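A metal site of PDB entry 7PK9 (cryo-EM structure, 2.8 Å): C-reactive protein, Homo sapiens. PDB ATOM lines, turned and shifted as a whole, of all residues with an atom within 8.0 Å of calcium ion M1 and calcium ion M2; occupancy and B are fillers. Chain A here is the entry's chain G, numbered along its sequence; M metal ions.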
ATOM      1  N   SER A  50     -18.241  20.455  15.204  1.00  0.00           N
ATOM      2  CA  SER A  50     -19.312  19.475  15.321  1.00  0.00           C
ATOM      3  C   SER A  50     -19.465  18.868  16.721  1.00  0.00           C
ATOM      4  O   SER A  50     -18.550  18.228  17.229  1.00  0.00           O
ATOM      5  CB  SER A  50     -19.083  18.353  14.321  1.00  0.00           C
ATOM      6  OG  SER A  50     -20.233  17.520  14.257  1.00  0.00           O
ATOM      7  N   SER A  53     -23.278  14.913  14.781  1.00  0.00           N
ATOM      8  CA  SER A  53     -23.429  14.819  13.340  1.00  0.00           C
ATOM      9  C   SER A  53     -24.246  13.568  13.002  1.00  0.00           C
ATOM     10  O   SER A  53     -23.810  12.440  13.248  1.00  0.00           O
ATOM     11  CB  SER A  53     -22.062  14.791  12.664  1.00  0.00           C
ATOM     12  OG  SER A  53     -22.179  14.897  11.263  1.00  0.00           O
ATOM     13  N   ALA A  55     -26.145  11.888   9.772  1.00  0.00           N
ATOM     14  CA  ALA A  55     -26.191  11.962   8.316  1.00  0.00           C
ATOM     15  C   ALA A  55     -26.869  10.734   7.728  1.00  0.00           C
ATOM     16  O   ALA A  55     -26.802   9.635   8.276  1.00  0.00           O
ATOM     17  CB  ALA A  55     -24.798  12.050   7.717  1.00  0.00           C
ATOM     18  N   GLN A  59     -28.695  13.045   2.889  1.00  0.00           N
ATOM     19  CA  GLN A  59     -28.438  14.339   3.533  1.00  0.00           C
ATOM     20  C   GLN A  59     -27.355  14.159   4.578  1.00  0.00           C
ATOM     21  O   GLN A  59     -27.566  13.455   5.573  1.00  0.00           O
ATOM     22  CB  GLN A  59     -29.728  14.841   4.160  1.00  0.00           C
ATOM     23  CG  GLN A  59     -29.612  16.120   4.939  1.00  0.00           C
ATOM     24  CD  GLN A  59     -28.963  17.219   4.138  1.00  0.00           C
ATOM     25  OE1 GLN A  59     -27.787  17.528   4.328  1.00  0.00           O
ATOM     26  NE2 GLN A  59     -29.726  17.808   3.228  1.00  0.00           N
ATOM     27  N   ASP A  60     -26.187  14.774   4.352  1.00  0.00           N
ATOM     28  CA  ASP A  60     -25.069  14.645   5.270  1.00  0.00           C
ATOM     29  C   ASP A  60     -25.278  15.423   6.558  1.00  0.00           C
ATOM     30  O   ASP A  60     -24.649  15.089   7.572  1.00  0.00           O
ATOM     31  CB  ASP A  60     -23.769  15.103   4.614  1.00  0.00           C
ATOM     32  CG  ASP A  60     -23.770  16.563   4.255  1.00  0.00           C
ATOM     33  OD1 ASP A  60     -24.806  17.224   4.468  1.00  0.00           O
ATOM     34  OD2 ASP A  60     -22.740  17.069   3.760  1.00  0.00           O
ATOM     35  N   ASN A  61     -26.132  16.438   6.556  1.00  0.00           N
ATOM     36  CA  ASN A  61     -26.423  17.208   7.755  1.00  0.00           C
ATOM     37  C   ASN A  61     -27.866  16.978   8.182  1.00  0.00           C
ATOM     38  O   ASN A  61     -28.646  17.926   8.295  1.00  0.00           O
ATOM     39  CB  ASN A  61     -26.202  18.704   7.513  1.00  0.00           C
ATOM     40  CG  ASN A  61     -24.770  19.036   7.221  1.00  0.00           C
ATOM     41  OD1 ASN A  61     -23.852  18.439   7.793  1.00  0.00           O
ATOM     42  ND2 ASN A  61     -24.553  20.013   6.359  1.00  0.00           N
ATOM     43  N   GLU A  62     -28.227  15.721   8.398  1.00  0.00           N
ATOM     44  CA  GLU A  62     -29.615  15.407   8.700  1.00  0.00           C
ATOM     45  C   GLU A  62     -29.987  15.829  10.109  1.00  0.00           C
ATOM     46  O   GLU A  62     -31.097  16.320  10.344  1.00  0.00           O
ATOM     47  CB  GLU A  62     -29.855  13.926   8.459  1.00  0.00           C
ATOM     48  CG  GLU A  62     -31.269  13.489   8.696  1.00  0.00           C
ATOM     49  CD  GLU A  62     -32.211  14.102   7.693  1.00  0.00           C
ATOM     50  OE1 GLU A  62     -31.751  14.442   6.589  1.00  0.00           O
ATOM     51  OE2 GLU A  62     -33.417  14.203   7.974  1.00  0.00           O
ATOM     52  N   LEU A  64     -27.479  18.193  12.746  1.00  0.00           N
ATOM     53  CA  LEU A  64     -26.182  18.777  13.094  1.00  0.00           C
ATOM     54  C   LEU A  64     -26.392  19.690  14.285  1.00  0.00           C
ATOM     55  O   LEU A  64     -27.063  20.718  14.162  1.00  0.00           O
ATOM     56  CB  LEU A  64     -25.567  19.524  11.912  1.00  0.00           C
ATOM     57  CG  LEU A  64     -24.090  19.869  12.013  1.00  0.00           C
ATOM     58  CD1 LEU A  64     -23.177  18.663  12.177  1.00  0.00           C
ATOM     59  CD2 LEU A  64     -23.681  20.680  10.817  1.00  0.00           C
ATOM     60  N   PHE A  66     -24.045  22.106  16.030  1.00  0.00           N
ATOM     61  CA  PHE A  66     -22.777  22.695  15.641  1.00  0.00           C
ATOM     62  C   PHE A  66     -22.577  24.024  16.368  1.00  0.00           C
ATOM     63  O   PHE A  66     -23.391  24.934  16.226  1.00  0.00           O
ATOM     64  CB  PHE A  66     -22.726  22.912  14.134  1.00  0.00           C
ATOM     65  CG  PHE A  66     -21.354  23.094  13.582  1.00  0.00           C
ATOM     66  CD1 PHE A  66     -20.671  22.035  13.021  1.00  0.00           C
ATOM     67  CD2 PHE A  66     -20.769  24.344  13.573  1.00  0.00           C
ATOM     68  CE1 PHE A  66     -19.417  22.219  12.505  1.00  0.00           C
ATOM     69  CE2 PHE A  66     -19.516  24.529  13.057  1.00  0.00           C
ATOM     70  CZ  PHE A  66     -18.831  23.464  12.517  1.00  0.00           C
ATOM     71  N   THR A  76     -29.423  22.177  12.979  1.00  0.00           N
ATOM     72  CA  THR A  76     -29.896  21.986  11.611  1.00  0.00           C
ATOM     73  C   THR A  76     -30.551  20.636  11.495  1.00  0.00           C
ATOM     74  O   THR A  76     -30.038  19.634  11.994  1.00  0.00           O
ATOM     75  CB  THR A  76     -28.762  22.026  10.574  1.00  0.00           C
ATOM     76  OG1 THR A  76     -27.946  20.861  10.724  1.00  0.00           O
ATOM     77  CG2 THR A  76     -27.901  23.211  10.765  1.00  0.00           C
ATOM     78  N   GLN A 137     -16.581  14.487  14.657  1.00  0.00           N
ATOM     79  CA  GLN A 137     -16.391  14.965  13.308  1.00  0.00           C
ATOM     80  C   GLN A 137     -17.720  15.493  12.795  1.00  0.00           C
ATOM     81  O   GLN A 137     -18.784  15.026  13.205  1.00  0.00           O
ATOM     82  CB  GLN A 137     -15.875  13.879  12.364  1.00  0.00           C
ATOM     83  CG  GLN A 137     -14.596  13.217  12.795  1.00  0.00           C
ATOM     84  CD  GLN A 137     -13.424  14.191  12.860  1.00  0.00           C
ATOM     85  OE1 GLN A 137     -13.463  15.252  12.243  1.00  0.00           O
ATOM     86  NE2 GLN A 137     -12.385  13.815  13.579  1.00  0.00           N
ATOM     87  N   GLU A 138     -17.654  16.449  11.886  1.00  0.00           N
ATOM     88  CA  GLU A 138     -18.765  16.746  10.987  1.00  0.00           C
ATOM     89  C   GLU A 138     -18.591  15.916   9.723  1.00  0.00           C
ATOM     90  O   GLU A 138     -17.563  16.004   9.051  1.00  0.00           O
ATOM     91  CB  GLU A 138     -18.816  18.235  10.691  1.00  0.00           C
ATOM     92  CG  GLU A 138     -20.172  18.731  10.250  1.00  0.00           C
ATOM     93  CD  GLU A 138     -20.342  18.610   8.766  1.00  0.00           C
ATOM     94  OE1 GLU A 138     -19.360  18.891   8.054  1.00  0.00           O
ATOM     95  OE2 GLU A 138     -21.438  18.223   8.303  1.00  0.00           O
ATOM     96  N   GLN A 139     -19.604  15.105   9.400  1.00  0.00           N
ATOM     97  CA  GLN A 139     -19.555  14.259   8.229  1.00  0.00           C
ATOM     98  C   GLN A 139     -20.272  14.933   7.060  1.00  0.00           C
ATOM     99  O   GLN A 139     -21.394  15.416   7.205  1.00  0.00           O
ATOM    100  CB  GLN A 139     -20.146  12.864   8.482  1.00  0.00           C
ATOM    101  CG  GLN A 139     -21.647  12.742   8.599  1.00  0.00           C
ATOM    102  CD  GLN A 139     -22.055  11.566   9.474  1.00  0.00           C
ATOM    103  OE1 GLN A 139     -21.851  10.424   9.107  1.00  0.00           O
ATOM    104  NE2 GLN A 139     -22.674  11.839  10.606  1.00  0.00           N
ATOM    105  N   ASP A 140     -19.586  14.978   5.919  1.00  0.00           N
ATOM    106  CA  ASP A 140     -20.083  15.603   4.699  1.00  0.00           C
ATOM    107  C   ASP A 140     -20.394  14.603   3.606  1.00  0.00           C
ATOM    108  O   ASP A 140     -20.976  14.992   2.586  1.00  0.00           O
ATOM    109  CB  ASP A 140     -19.072  16.617   4.162  1.00  0.00           C
ATOM    110  CG  ASP A 140     -18.956  17.831   5.025  1.00  0.00           C
ATOM    111  OD1 ASP A 140     -19.704  17.895   6.010  1.00  0.00           O
ATOM    112  OD2 ASP A 140     -18.142  18.723   4.723  1.00  0.00           O
ATOM    113  N   SER A 141     -20.015  13.355   3.780  1.00  0.00           N
ATOM    114  CA  SER A 141     -20.617  12.245   3.067  1.00  0.00           C
ATOM    115  C   SER A 141     -21.433  11.447   4.070  1.00  0.00           C
ATOM    116  O   SER A 141     -21.610  11.854   5.229  1.00  0.00           O
ATOM    117  CB  SER A 141     -19.535  11.403   2.409  1.00  0.00           C
ATOM    118  OG  SER A 141     -18.652  10.886   3.392  1.00  0.00           O
ATOM    119  N   GLY A 144     -18.187  10.050   6.105  1.00  0.00           N
ATOM    120  CA  GLY A 144     -16.829  10.500   5.894  1.00  0.00           C
ATOM    121  C   GLY A 144     -16.753  11.940   5.437  1.00  0.00           C
ATOM    122  O   GLY A 144     -17.691  12.719   5.634  1.00  0.00           O
ATOM    123  N   ASN A 145     -15.633  12.270   4.798  1.00  0.00           N
ATOM    124  CA  ASN A 145     -15.344  13.632   4.347  1.00  0.00           C
ATOM    125  C   ASN A 145     -15.281  14.608   5.519  1.00  0.00           C
ATOM    126  O   ASN A 145     -15.729  15.748   5.427  1.00  0.00           O
ATOM    127  CB  ASN A 145     -16.370  14.107   3.320  1.00  0.00           C
ATOM    128  CG  ASN A 145     -16.414  13.221   2.097  1.00  0.00           C
ATOM    129  OD1 ASN A 145     -16.728  12.034   2.180  1.00  0.00           O
ATOM    130  ND2 ASN A 145     -16.116  13.800   0.950  1.00  0.00           N
ATOM    131  N   PHE A 146     -14.721  14.148   6.628  1.00  0.00           N
ATOM    132  CA  PHE A 146     -14.497  14.988   7.794  1.00  0.00           C
ATOM    133  C   PHE A 146     -13.535  16.134   7.464  1.00  0.00           C
ATOM    134  O   PHE A 146     -12.771  16.086   6.516  1.00  0.00           O
ATOM    135  CB  PHE A 146     -13.986  14.157   8.969  1.00  0.00           C
ATOM    136  CG  PHE A 146     -14.652  12.821   9.109  1.00  0.00           C
ATOM    137  CD1 PHE A 146     -16.022  12.739   9.252  1.00  0.00           C
ATOM    138  CD2 PHE A 146     -13.925  11.661   9.084  1.00  0.00           C
ATOM    139  CE1 PHE A 146     -16.647  11.531   9.392  1.00  0.00           C
ATOM    140  CE2 PHE A 146     -14.532  10.449   9.213  1.00  0.00           C
ATOM    141  CZ  PHE A 146     -15.899  10.379   9.363  1.00  0.00           C
ATOM    142  N   GLU A 147     -13.623  17.188   8.273  1.00  0.00           N
ATOM    143  CA  GLU A 147     -12.745  18.360   8.166  1.00  0.00           C
ATOM    144  C   GLU A 147     -12.110  18.620   9.519  1.00  0.00           C
ATOM    145  O   GLU A 147     -12.804  18.832  10.509  1.00  0.00           O
ATOM    146  CB  GLU A 147     -13.527  19.578   7.694  1.00  0.00           C
ATOM    147  CG  GLU A 147     -14.151  19.405   6.324  1.00  0.00           C
ATOM    148  CD  GLU A 147     -15.302  20.361   6.096  1.00  0.00           C
ATOM    149  OE1 GLU A 147     -16.443  19.874   6.017  1.00  0.00           O
ATOM    150  OE2 GLU A 147     -15.058  21.575   5.997  1.00  0.00           O
ATOM    151  N   SER A 149     -10.606  21.206  10.763  1.00  0.00           N
ATOM    152  CA  SER A 149     -11.129  22.441  11.330  1.00  0.00           C
ATOM    153  C   SER A 149     -12.504  22.291  11.990  1.00  0.00           C
ATOM    154  O   SER A 149     -12.929  23.221  12.684  1.00  0.00           O
ATOM    155  CB  SER A 149     -11.219  23.504  10.248  1.00  0.00           C
ATOM    156  OG  SER A 149     -12.140  23.117   9.246  1.00  0.00           O
ATOM    157  N   GLN A 150     -13.205  21.184  11.772  1.00  0.00           N
ATOM    158  CA  GLN A 150     -14.519  20.950  12.358  1.00  0.00           C
ATOM    159  C   GLN A 150     -14.546  19.798  13.339  1.00  0.00           C
ATOM    160  O   GLN A 150     -15.605  19.517  13.908  1.00  0.00           O
ATOM    161  CB  GLN A 150     -15.546  20.740  11.255  1.00  0.00           C
ATOM    162  CG  GLN A 150     -15.603  21.873  10.278  1.00  0.00           C
ATOM    163  CD  GLN A 150     -16.771  21.758   9.341  1.00  0.00           C
ATOM    164  OE1 GLN A 150     -17.216  20.666   9.014  1.00  0.00           O
ATOM    165  NE2 GLN A 150     -17.304  22.895   8.932  1.00  0.00           N
HETATM  166 CA    CA M   1     -18.208  20.494   7.067  1.00  0.00          CA
HETATM  167 CA    CA M   2     -21.896  18.913   6.232  1.00  0.00          CA
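OD1 of Asp 60 sits close to OE1 of Gln 59, 3.0 Å away. OE1 of Gln 59 sits at hydrogen-bond distance from N of Asn 61, at 3.0 Å. The backbone NH (N) of Ser 50 lies within hydrogen-bond range of the backbone carbonyl oxygen (O) of Gln 150 (3.1 Å). The backbone carbonyl oxygen (O) of Ser 53 lies within hydrogen-bond range of the side-chain amide nitrogen (NE2) of Gln 139 (2.9 Å). OE1 of Glu 147 sits close to OD2 of Asp 140, at 2.4 Å. OD1 of Asp 60 lies close to ND2 of Asn 61 (3.4 Å).
Residues that only touch calcium ion M2: Asp 60 (3.2 Å) and Gln 139 (3.7 Å). Of the 21 residues printed, 5 come within 4 Å of calcium ion M2. The nearest printed residue that does not touch calcium ion M2 is Leu 64 (5.2 Å).
The side-chain carboxylate (OE1) of Glu 147 binds calcium ion M1 (2.1 Å). OE1 of Gln 150 is bound to calcium ion M1 (2.2 Å). The side-chain carboxylate (OE1) of Glu 138 is bound to calcium ion M1 (2.2 Å). Calcium ion M1 has three donor atoms within binding distance. Slightly farther from calcium ion M1 lies the side-chain carboxylate (OD2) of Asp 140 (2.9 Å).
Calcium ion M2 is bound by OE2 of Glu 138 (2.2 Å), OD1 of Asp 140 (2.4 Å), OD1 of Asn 61 (2.5 Å) and ND2 of Asn 61 (2.9 Å). Calcium ion M2 has four donor atoms within binding distance. Slightly farther from calcium ion M2 lies the side-chain carboxylate (OE1) of Glu 138 (3.1 Å).
Of the 21 residues printed, 4 come within 4 Å of calcium ion M1. The nearest printed residue that does not touch calcium ion M1 is Asn 145 (5.6 Å).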
